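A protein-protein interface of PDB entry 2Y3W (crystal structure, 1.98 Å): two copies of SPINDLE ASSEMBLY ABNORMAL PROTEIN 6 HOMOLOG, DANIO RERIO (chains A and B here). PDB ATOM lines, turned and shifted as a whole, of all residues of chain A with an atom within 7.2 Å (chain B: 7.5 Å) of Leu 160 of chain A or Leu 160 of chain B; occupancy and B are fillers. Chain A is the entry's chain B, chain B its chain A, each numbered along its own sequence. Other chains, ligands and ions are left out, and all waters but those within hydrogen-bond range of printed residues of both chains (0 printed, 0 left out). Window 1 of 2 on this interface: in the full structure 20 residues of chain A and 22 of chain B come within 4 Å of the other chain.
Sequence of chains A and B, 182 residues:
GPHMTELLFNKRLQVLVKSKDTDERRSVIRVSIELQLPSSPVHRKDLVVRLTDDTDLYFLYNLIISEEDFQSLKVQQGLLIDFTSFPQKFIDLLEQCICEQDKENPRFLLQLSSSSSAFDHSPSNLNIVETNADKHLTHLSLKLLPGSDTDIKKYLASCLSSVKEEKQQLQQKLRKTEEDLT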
ATOM      1  N   ASP A  54     -19.450 -22.948 -29.209  1.00  0.00           N
ATOM      2  CA  ASP A  54     -19.529 -21.487 -29.259  1.00  0.00           C
ATOM      3  C   ASP A  54     -20.790 -20.882 -28.632  1.00  0.00           C
ATOM      4  O   ASP A  54     -20.848 -19.676 -28.416  1.00  0.00           O
ATOM      5  CB  ASP A  54     -19.390 -20.985 -30.698  1.00  0.00           C
ATOM      6  CG  ASP A  54     -17.979 -21.111 -31.223  1.00  0.00           C
ATOM      7  OD1 ASP A  54     -17.085 -21.467 -30.433  1.00  0.00           O
ATOM      8  OD2 ASP A  54     -17.763 -20.848 -32.426  1.00  0.00           O
ATOM      9  N   LEU A  57     -21.955 -22.720 -23.403  1.00  0.00           N
ATOM     10  CA  LEU A  57     -20.710 -22.392 -22.719  1.00  0.00           C
ATOM     11  C   LEU A  57     -20.356 -23.390 -21.621  1.00  0.00           C
ATOM     12  O   LEU A  57     -19.266 -23.336 -21.058  1.00  0.00           O
ATOM     13  CB  LEU A  57     -20.786 -20.970 -22.150  1.00  0.00           C
ATOM     14  CG  LEU A  57     -21.009 -19.856 -23.179  1.00  0.00           C
ATOM     15  CD1 LEU A  57     -21.089 -18.489 -22.508  1.00  0.00           C
ATOM     16  CD2 LEU A  57     -19.916 -19.876 -24.237  1.00  0.00           C
ATOM     17  N   LYS A 153     -14.508 -23.529 -15.521  1.00  0.00           N
ATOM     18  CA  LYS A 153     -14.157 -22.236 -14.945  1.00  0.00           C
ATOM     19  C   LYS A 153     -12.870 -21.704 -15.563  1.00  0.00           C
ATOM     20  O   LYS A 153     -12.819 -20.554 -16.008  1.00  0.00           O
ATOM     21  CB  LYS A 153     -14.012 -22.328 -13.422  1.00  0.00           C
ATOM     22  CG  LYS A 153     -13.450 -21.066 -12.784  1.00  0.00           C
ATOM     23  CD  LYS A 153     -13.156 -21.254 -11.296  1.00  0.00           C
ATOM     24  CE  LYS A 153     -11.977 -22.192 -11.079  1.00  0.00           C
ATOM     25  NZ  LYS A 153     -11.564 -22.233  -9.650  1.00  0.00           N
ATOM     26  N   LYS A 154     -11.832 -22.537 -15.582  1.00  0.00           N
ATOM     27  CA  LYS A 154     -10.546 -22.157 -16.164  1.00  0.00           C
ATOM     28  C   LYS A 154     -10.662 -21.827 -17.653  1.00  0.00           C
ATOM     29  O   LYS A 154     -10.090 -20.845 -18.118  1.00  0.00           O
ATOM     30  CB  LYS A 154      -9.493 -23.257 -15.952  1.00  0.00           C
ATOM     31  CG  LYS A 154      -9.034 -23.410 -14.512  1.00  0.00           C
ATOM     32  CD  LYS A 154      -8.186 -24.668 -14.327  1.00  0.00           C
ATOM     33  CE  LYS A 154      -7.736 -24.829 -12.882  1.00  0.00           C
ATOM     34  NZ  LYS A 154      -7.109 -26.160 -12.636  1.00  0.00           N
ATOM     35  N   TYR A 155     -11.402 -22.644 -18.397  1.00  0.00           N
ATOM     36  CA  TYR A 155     -11.582 -22.394 -19.825  1.00  0.00           C
ATOM     37  C   TYR A 155     -12.316 -21.075 -20.084  1.00  0.00           C
ATOM     38  O   TYR A 155     -11.909 -20.279 -20.926  1.00  0.00           O
ATOM     39  CB  TYR A 155     -12.327 -23.541 -20.509  1.00  0.00           C
ATOM     40  CG  TYR A 155     -12.502 -23.290 -21.989  1.00  0.00           C
ATOM     41  CD1 TYR A 155     -11.402 -23.251 -22.831  1.00  0.00           C
ATOM     42  CD2 TYR A 155     -13.759 -23.064 -22.539  1.00  0.00           C
ATOM     43  CE1 TYR A 155     -11.543 -23.003 -24.177  1.00  0.00           C
ATOM     44  CE2 TYR A 155     -13.909 -22.816 -23.893  1.00  0.00           C
ATOM     45  CZ  TYR A 155     -12.795 -22.791 -24.704  1.00  0.00           C
ATOM     46  OH  TYR A 155     -12.916 -22.547 -26.052  1.00  0.00           O
ATOM     47  N   LEU A 156     -13.394 -20.843 -19.347  1.00  0.00           N
ATOM     48  CA  LEU A 156     -14.140 -19.600 -19.491  1.00  0.00           C
ATOM     49  C   LEU A 156     -13.238 -18.397 -19.230  1.00  0.00           C
ATOM     50  O   LEU A 156     -13.279 -17.411 -19.957  1.00  0.00           O
ATOM     51  CB  LEU A 156     -15.356 -19.594 -18.566  1.00  0.00           C
ATOM     52  CG  LEU A 156     -16.418 -20.637 -18.942  1.00  0.00           C
ATOM     53  CD1 LEU A 156     -17.597 -20.591 -17.988  1.00  0.00           C
ATOM     54  CD2 LEU A 156     -16.894 -20.453 -20.374  1.00  0.00           C
ATOM     55  N   ALA A 157     -12.413 -18.483 -18.196  1.00  0.00           N
ATOM     56  CA  ALA A 157     -11.483 -17.403 -17.877  1.00  0.00           C
ATOM     57  C   ALA A 157     -10.533 -17.104 -19.034  1.00  0.00           C
ATOM     58  O   ALA A 157     -10.286 -15.939 -19.356  1.00  0.00           O
ATOM     59  CB  ALA A 157     -10.704 -17.720 -16.607  1.00  0.00           C
ATOM     60  N   SER A 158     -10.008 -18.149 -19.670  1.00  0.00           N
ATOM     61  CA  SER A 158      -9.114 -17.945 -20.809  1.00  0.00           C
ATOM     62  C   SER A 158      -9.864 -17.371 -22.015  1.00  0.00           C
ATOM     63  O   SER A 158      -9.313 -16.575 -22.774  1.00  0.00           O
ATOM     64  CB  SER A 158      -8.376 -19.235 -21.182  1.00  0.00           C
ATOM     65  OG  SER A 158      -9.239 -20.183 -21.780  1.00  0.00           O
ATOM     66  N   CYS A 159     -11.120 -17.771 -22.186  1.00  0.00           N
ATOM     67  CA  CYS A 159     -11.978 -17.190 -23.221  1.00  0.00           C
ATOM     68  C   CYS A 159     -12.249 -15.703 -22.988  1.00  0.00           C
ATOM     69  O   CYS A 159     -12.207 -14.908 -23.925  1.00  0.00           O
ATOM     70  CB  CYS A 159     -13.310 -17.935 -23.312  1.00  0.00           C
ATOM     71  SG  CYS A 159     -13.215 -19.539 -24.114  1.00  0.00           S
ATOM     72  N   LEU A 160     -12.544 -15.339 -21.745  1.00  0.00           N
ATOM     73  CA  LEU A 160     -12.749 -13.939 -21.388  1.00  0.00           C
ATOM     74  C   LEU A 160     -11.526 -13.082 -21.698  1.00  0.00           C
ATOM     75  O   LEU A 160     -11.653 -11.958 -22.180  1.00  0.00           O
ATOM     76  CB  LEU A 160     -13.125 -13.806 -19.912  1.00  0.00           C
ATOM     77  CG  LEU A 160     -14.604 -14.032 -19.596  1.00  0.00           C
ATOM     78  CD1 LEU A 160     -14.796 -14.329 -18.117  1.00  0.00           C
ATOM     79  CD2 LEU A 160     -15.444 -12.835 -20.032  1.00  0.00           C
ATOM     80  N   SER A 161     -10.339 -13.605 -21.411  1.00  0.00           N
ATOM     81  CA  SER A 161      -9.117 -12.868 -21.690  1.00  0.00           C
ATOM     82  C   SER A 161      -8.933 -12.633 -23.187  1.00  0.00           C
ATOM     83  O   SER A 161      -8.635 -11.521 -23.619  1.00  0.00           O
ATOM     84  CB  SER A 161      -7.898 -13.588 -21.110  1.00  0.00           C
ATOM     85  OG  SER A 161      -7.900 -13.512 -19.696  1.00  0.00           O
ATOM     86  N   SER A 162      -9.127 -13.684 -23.975  1.00  0.00           N
ATOM     87  CA  SER A 162      -8.908 -13.593 -25.414  1.00  0.00           C
ATOM     88  C   SER A 162      -9.919 -12.687 -26.123  1.00  0.00           C
ATOM     89  O   SER A 162      -9.543 -11.900 -26.986  1.00  0.00           O
ATOM     90  CB  SER A 162      -8.889 -14.985 -26.052  1.00  0.00           C
ATOM     91  OG  SER A 162     -10.052 -15.714 -25.712  1.00  0.00           O
ATOM     92  N   VAL A 163     -11.194 -12.799 -25.765  1.00  0.00           N
ATOM     93  CA  VAL A 163     -12.213 -11.953 -26.373  1.00  0.00           C
ATOM     94  C   VAL A 163     -11.998 -10.485 -26.005  1.00  0.00           C
ATOM     95  O   VAL A 163     -12.225  -9.592 -26.821  1.00  0.00           O
ATOM     96  CB  VAL A 163     -13.643 -12.373 -25.978  1.00  0.00           C
ATOM     97  CG1 VAL A 163     -14.647 -11.392 -26.546  1.00  0.00           C
ATOM     98  CG2 VAL A 163     -13.944 -13.772 -26.481  1.00  0.00           C
ATOM     99  N   LYS A 164     -11.568 -10.237 -24.774  1.00  0.00           N
ATOM    100  CA  LYS A 164     -11.240  -8.883 -24.365  1.00  0.00           C
ATOM    101  C   LYS A 164     -10.083  -8.322 -25.189  1.00  0.00           C
ATOM    102  O   LYS A 164     -10.091  -7.151 -25.570  1.00  0.00           O
ATOM    103  CB  LYS A 164     -10.943  -8.823 -22.864  1.00  0.00           C
ATOM    104  CG  LYS A 164     -12.214  -8.650 -22.032  1.00  0.00           C
ATOM    105  CD  LYS A 164     -12.027  -9.030 -20.571  1.00  0.00           C
ATOM    106  CE  LYS A 164     -13.343  -8.901 -19.812  1.00  0.00           C
ATOM    107  NZ  LYS A 164     -13.261  -9.451 -18.433  1.00  0.00           N
ATOM    108  N   GLU A 165      -9.101  -9.165 -25.478  1.00  0.00           N
ATOM    109  CA  GLU A 165      -7.965  -8.750 -26.288  1.00  0.00           C
ATOM    110  C   GLU A 165      -8.415  -8.420 -27.707  1.00  0.00           C
ATOM    111  O   GLU A 165      -7.966  -7.438 -28.295  1.00  0.00           O
ATOM    112  CB  GLU A 165      -6.885  -9.834 -26.299  1.00  0.00           C
ATOM    113  CG  GLU A 165      -5.542  -9.364 -26.826  1.00  0.00           C
ATOM    114  CD  GLU A 165      -4.437 -10.385 -26.604  1.00  0.00           C
ATOM    115  OE1 GLU A 165      -4.748 -11.590 -26.468  1.00  0.00           O
ATOM    116  OE2 GLU A 165      -3.256  -9.976 -26.562  1.00  0.00           O
ATOM    117  N   GLU A 166      -9.303  -9.239 -28.259  1.00  0.00           N
ATOM    118  CA  GLU A 166      -9.877  -8.954 -29.569  1.00  0.00           C
ATOM    119  C   GLU A 166     -10.694  -7.663 -29.533  1.00  0.00           C
ATOM    120  O   GLU A 166     -10.624  -6.848 -30.459  1.00  0.00           O
ATOM    121  CB  GLU A 166     -10.755 -10.114 -30.039  1.00  0.00           C
ATOM    122  CG  GLU A 166     -10.051 -11.469 -30.056  1.00  0.00           C
ATOM    123  CD  GLU A 166     -10.917 -12.573 -30.643  1.00  0.00           C
ATOM    124  OE1 GLU A 166     -12.045 -12.273 -31.086  1.00  0.00           O
ATOM    125  OE2 GLU A 166     -10.470 -13.742 -30.663  1.00  0.00           O
ATOM    126  N   LEU B  57     -10.764 -12.739 -11.535  1.00  0.00           N
ATOM    127  CA  LEU B  57     -11.939 -13.429 -12.037  1.00  0.00           C
ATOM    128  C   LEU B  57     -12.370 -14.571 -11.124  1.00  0.00           C
ATOM    129  O   LEU B  57     -13.444 -15.133 -11.301  1.00  0.00           O
ATOM    130  CB  LEU B  57     -11.697 -13.952 -13.460  1.00  0.00           C
ATOM    131  CG  LEU B  57     -11.549 -12.898 -14.559  1.00  0.00           C
ATOM    132  CD1 LEU B  57     -11.600 -13.554 -15.922  1.00  0.00           C
ATOM    133  CD2 LEU B  57     -12.636 -11.844 -14.453  1.00  0.00           C
ATOM    134  N   ILE B 152     -18.856 -19.706  -9.726  1.00  0.00           N
ATOM    135  CA  ILE B 152     -17.929 -18.932 -10.538  1.00  0.00           C
ATOM    136  C   ILE B 152     -18.109 -19.256 -12.026  1.00  0.00           C
ATOM    137  O   ILE B 152     -18.043 -18.372 -12.879  1.00  0.00           O
ATOM    138  CB  ILE B 152     -16.465 -19.174 -10.105  1.00  0.00           C
ATOM    139  CG1 ILE B 152     -16.266 -18.749  -8.643  1.00  0.00           C
ATOM    140  CG2 ILE B 152     -15.506 -18.413 -11.018  1.00  0.00           C
ATOM    141  CD1 ILE B 152     -14.894 -19.076  -8.081  1.00  0.00           C
ATOM    142  N   LYS B 154     -20.887 -20.205 -13.480  1.00  0.00           N
ATOM    143  CA  LYS B 154     -22.103 -19.519 -13.894  1.00  0.00           C
ATOM    144  C   LYS B 154     -21.829 -18.044 -14.154  1.00  0.00           C
ATOM    145  O   LYS B 154     -22.281 -17.489 -15.153  1.00  0.00           O
ATOM    146  CB  LYS B 154     -23.202 -19.673 -12.844  1.00  0.00           C
ATOM    147  CG  LYS B 154     -23.687 -21.099 -12.657  1.00  0.00           C
ATOM    148  CD  LYS B 154     -24.715 -21.183 -11.533  1.00  0.00           C
ATOM    149  CE  LYS B 154     -25.176 -22.618 -11.314  1.00  0.00           C
ATOM    150  NZ  LYS B 154     -26.088 -22.730 -10.132  1.00  0.00           N
ATOM    151  N   TYR B 155     -21.075 -17.411 -13.260  1.00  0.00           N
ATOM    152  CA  TYR B 155     -20.797 -15.989 -13.412  1.00  0.00           C
ATOM    153  C   TYR B 155     -19.905 -15.689 -14.618  1.00  0.00           C
ATOM    154  O   TYR B 155     -20.211 -14.800 -15.410  1.00  0.00           O
ATOM    155  CB  TYR B 155     -20.203 -15.376 -12.137  1.00  0.00           C
ATOM    156  CG  TYR B 155     -19.943 -13.899 -12.299  1.00  0.00           C
ATOM    157  CD1 TYR B 155     -20.990 -13.019 -12.539  1.00  0.00           C
ATOM    158  CD2 TYR B 155     -18.657 -13.386 -12.249  1.00  0.00           C
ATOM    159  CE1 TYR B 155     -20.765 -11.665 -12.712  1.00  0.00           C
ATOM    160  CE2 TYR B 155     -18.419 -12.029 -12.424  1.00  0.00           C
ATOM    161  CZ  TYR B 155     -19.482 -11.174 -12.652  1.00  0.00           C
ATOM    162  OH  TYR B 155     -19.266  -9.826 -12.827  1.00  0.00           O
ATOM    163  N   LEU B 156     -18.808 -16.430 -14.759  1.00  0.00           N
ATOM    164  CA  LEU B 156     -17.911 -16.249 -15.895  1.00  0.00           C
ATOM    165  C   LEU B 156     -18.632 -16.478 -17.227  1.00  0.00           C
ATOM    166  O   LEU B 156     -18.376 -15.778 -18.210  1.00  0.00           O
ATOM    167  CB  LEU B 156     -16.683 -17.158 -15.777  1.00  0.00           C
ATOM    168  CG  LEU B 156     -15.768 -16.859 -14.583  1.00  0.00           C
ATOM    169  CD1 LEU B 156     -14.549 -17.763 -14.598  1.00  0.00           C
ATOM    170  CD2 LEU B 156     -15.352 -15.404 -14.593  1.00  0.00           C
ATOM    171  N   ALA B 157     -19.543 -17.442 -17.254  1.00  0.00           N
ATOM    172  CA  ALA B 157     -20.318 -17.697 -18.465  1.00  0.00           C
ATOM    173  C   ALA B 157     -21.200 -16.491 -18.815  1.00  0.00           C
ATOM    174  O   ALA B 157     -21.299 -16.110 -19.979  1.00  0.00           O
ATOM    175  CB  ALA B 157     -21.153 -18.965 -18.327  1.00  0.00           C
ATOM    176  N   SER B 158     -21.833 -15.891 -17.806  1.00  0.00           N
ATOM    177  CA  SER B 158     -22.627 -14.683 -18.017  1.00  0.00           C
ATOM    178  C   SER B 158     -21.761 -13.577 -18.597  1.00  0.00           C
ATOM    179  O   SER B 158     -22.154 -12.904 -19.555  1.00  0.00           O
ATOM    180  CB  SER B 158     -23.265 -14.203 -16.705  1.00  0.00           C
ATOM    181  OG  SER B 158     -24.225 -15.133 -16.237  1.00  0.00           O
ATOM    182  N   CYS B 159     -20.582 -13.391 -18.004  1.00  0.00           N
ATOM    183  CA  CYS B 159     -19.645 -12.373 -18.465  1.00  0.00           C
ATOM    184  C   CYS B 159     -19.193 -12.620 -19.897  1.00  0.00           C
ATOM    185  O   CYS B 159     -19.070 -11.683 -20.688  1.00  0.00           O
ATOM    186  CB  CYS B 159     -18.424 -12.287 -17.544  1.00  0.00           C
ATOM    187  SG  CYS B 159     -18.786 -11.631 -15.887  1.00  0.00           S
ATOM    188  N   LEU B 160     -18.932 -13.879 -20.229  1.00  0.00           N
ATOM    189  CA  LEU B 160     -18.456 -14.211 -21.566  1.00  0.00           C
ATOM    190  C   LEU B 160     -19.516 -13.889 -22.618  1.00  0.00           C
ATOM    191  O   LEU B 160     -19.209 -13.293 -23.645  1.00  0.00           O
ATOM    192  CB  LEU B 160     -18.036 -15.681 -21.651  1.00  0.00           C
ATOM    193  CG  LEU B 160     -17.453 -16.136 -22.993  1.00  0.00           C
ATOM    194  CD1 LEU B 160     -16.266 -15.274 -23.414  1.00  0.00           C
ATOM    195  CD2 LEU B 160     -17.060 -17.612 -22.940  1.00  0.00           C
ATOM    196  N   SER B 161     -20.753 -14.301 -22.365  1.00  0.00           N
ATOM    197  CA  SER B 161     -21.854 -14.015 -23.277  1.00  0.00           C
ATOM    198  C   SER B 161     -21.979 -12.512 -23.495  1.00  0.00           C
ATOM    199  O   SER B 161     -22.136 -12.050 -24.624  1.00  0.00           O
ATOM    200  CB  SER B 161     -23.168 -14.556 -22.717  1.00  0.00           C
ATOM    201  OG  SER B 161     -23.111 -15.965 -22.587  1.00  0.00           O
ATOM    202  N   SER B 162     -21.897 -11.752 -22.406  1.00  0.00           N
ATOM    203  CA  SER B 162     -21.962 -10.295 -22.485  1.00  0.00           C
ATOM    204  C   SER B 162     -20.841  -9.707 -23.318  1.00  0.00           C
ATOM    205  O   SER B 162     -21.086  -8.872 -24.189  1.00  0.00           O
ATOM    206  CB  SER B 162     -21.948  -9.664 -21.087  1.00  0.00           C
ATOM    207  OG  SER B 162     -23.174  -9.901 -20.427  1.00  0.00           O
ATOM    208  N   VAL B 163     -19.609 -10.125 -23.052  1.00  0.00           N
ATOM    209  CA  VAL B 163     -18.477  -9.577 -23.783  1.00  0.00           C
ATOM    210  C   VAL B 163     -18.533  -9.942 -25.281  1.00  0.00           C
ATOM    211  O   VAL B 163     -18.139  -9.152 -26.143  1.00  0.00           O
ATOM    212  CB  VAL B 163     -17.135 -10.005 -23.151  1.00  0.00           C
ATOM    213  CG1 VAL B 163     -15.969  -9.488 -23.958  1.00  0.00           C
ATOM    214  CG2 VAL B 163     -17.048  -9.491 -21.715  1.00  0.00           C
ATOM    215  N   LYS B 164     -19.044 -11.126 -25.595  1.00  0.00           N
ATOM    216  CA  LYS B 164     -19.162 -11.526 -26.999  1.00  0.00           C
ATOM    217  C   LYS B 164     -20.222 -10.702 -27.726  1.00  0.00           C
ATOM    218  O   LYS B 164     -20.046 -10.339 -28.884  1.00  0.00           O
ATOM    219  CB  LYS B 164     -19.456 -13.023 -27.120  1.00  0.00           C
ATOM    220  CG  LYS B 164     -18.254 -13.907 -26.777  1.00  0.00           C
ATOM    221  CD  LYS B 164     -18.669 -15.350 -26.519  1.00  0.00           C
ATOM    222  CE  LYS B 164     -19.181 -16.026 -27.776  1.00  0.00           C
ATOM    223  NZ  LYS B 164     -19.529 -17.458 -27.523  1.00  0.00           N
ATOM    224  N   GLU B 165     -21.324 -10.407 -27.045  1.00  0.00           N
ATOM    225  CA  GLU B 165     -22.344  -9.521 -27.593  1.00  0.00           C
ATOM    226  C   GLU B 165     -21.756  -8.131 -27.831  1.00  0.00           C
ATOM    227  O   GLU B 165     -21.996  -7.510 -28.863  1.00  0.00           O
ATOM    228  CB  GLU B 165     -23.552  -9.423 -26.652  1.00  0.00           C
ATOM    229  CG  GLU B 165     -24.539  -8.325 -27.040  1.00  0.00           C
ATOM    230  CD  GLU B 165     -25.477  -7.922 -25.906  1.00  0.00           C
ATOM    231  OE1 GLU B 165     -25.999  -8.813 -25.208  1.00  0.00           O
ATOM    232  OE2 GLU B 165     -25.696  -6.708 -25.716  1.00  0.00           O
ATOM    233  N   GLU B 166     -20.975  -7.652 -26.865  1.00  0.00           N
ATOM    234  CA  GLU B 166     -20.312  -6.359 -26.986  1.00  0.00           C
ATOM    235  C   GLU B 166     -19.364  -6.334 -28.179  1.00  0.00           C
ATOM    236  O   GLU B 166     -19.353  -5.375 -28.961  1.00  0.00           O
ATOM    237  CB  GLU B 166     -19.559  -6.022 -25.695  1.00  0.00           C
ATOM    238  CG  GLU B 166     -18.666  -4.798 -25.795  1.00  0.00           C
ATOM    239  CD  GLU B 166     -19.349  -3.510 -25.358  1.00  0.00           C
ATOM    240  OE1 GLU B 166     -20.569  -3.512 -25.085  1.00  0.00           O
ATOM    241  OE2 GLU B 166     -18.651  -2.482 -25.296  1.00  0.00           O
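The side-chain amino group of Lys 164 of chain B sits at hydrogen-bond distance from the backbone carbonyl oxygen of Asp 54 of chain A, at 2.7 Å.
The backbone carbonyl oxygen (O) of Ala 157 of chain B lies within hydrogen-bond range of the side-chain hydroxyl (OG) of Ser 161 of chain B (3.2 Å).
The backbone carbonyl oxygen (O) of Tyr 155 of chain A lies close to the side-chain sulfur (SG) of Cys 159 of chain A.
O of Cys 159 of chain A sits at hydrogen-bond distance from OG of Ser 162 of chain A, at 2.9 Å.
The side-chain sulfur (SG) of Cys 159 of chain B lies close to the backbone carbonyl oxygen (O) of Tyr 155 of chain B (3.5 Å).
Ala 157 of chain B touches Leu 57 of chain A.
Leu 160 of chain B touches Leu 57 of chain A.
OG of Ser 161 of chain B touches CD1 of Leu 57 of chain A, 3.2 Å away.
Ile 152 of chain B touches Lys 153 of chain A (CG2 to CD, 3.7 Å).
Leu 156 of chain B touches Lys 153 of chain A (CD1 to O, 3.6 Å).
CB of Leu 156 of chain A touches CB of Leu 156 of chain B (3.9 Å).
CD1 of Leu 156 of chain A touches N of Ala 157 of chain B (3.8 Å).
Leu 160 of chain B touches Leu 156 of chain A (CD2 to CD2, 3.8 Å).
Leu 160 of chain B touches Cys 159 of chain A (CD2 to CB, 3.8 Å).
CD1 of Leu 57 of chain B touches CD1 of Leu 160 of chain A, 3.95 Å away.
Lys 154 of chain A touches none of the printed residues of chain B.
Ser 158 of chain A touches none of the printed residues of chain B.
Leu 160 of chain A touches just these residues of chain B: Leu 57, Leu 156, Cys 159 and Leu 160.
Of the printed residues of chain A, Leu 57 of chain B touches Leu 160.
Leu 160 of chain B touches just these residues of chain A: Leu 57 (3.9 Å), Leu 156 (3.8 Å), Cys 159 (3.8 Å) and Leu 160 (3.6 Å).
Printed residues of chain A within 4 Å of Lys 164 of chain B: Asp 54 (2.7 Å).
The nearest residue of chain B that does not touch Leu 160 of chain A is Val 163 of chain B (4.1 Å).
The nearest residue of chain A that does not touch Leu 160 of chain B is Val 163 of chain A (4.1 Å).
The nearest printed residue of chain A that does not touch Ile 152 of chain B is Leu 156 of chain A (5.6 Å).
Printed residues of chain A that touch a printed residue of chain B: Asp 54, Leu 57, Lys 153, Leu 156, Cys 159, Leu 160 and Val 163.
Of the 15 printed residues of chain B, 9 touch a printed residue of chain A.
Printed residues of chain B that touch a printed residue of chain A: Leu 57, Ile 152, Leu 156, Ala 157, Cys 159, Leu 160, Ser 161, Val 163 and Lys 164.
Among the printed residues, 15 pairs touch across the chains.
Among the printed residues, no Asp or Glu carboxylate lies within 4 Å of a Lys or Arg side-chain nitrogen of the other chain.
Leu 156 of chain A touches Ala 157 of chain B, but with the chains exchanged Ala 157 of chain A does not touch Leu 156 of chain B (4.2 Å).
Cys 159 of chain A touches Leu 160 of chain B, and with the chains exchanged Leu 160 of chain A touches Cys 159 of chain B.
Leu 160 of chain B touches its own counterpart, Leu 160 of chain A.
Val 163 of chain A touches its own counterpart, Val 163 of chain B.
Positions printed for both chains: 57, 154, 155, 156, 157, 158, 159, 160, 161, 162, 163, 164, 165 and 166.
Of the 15 pairs that touch across the chains among the printed residues, 9 have their exchanged pair printed and touching as well.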
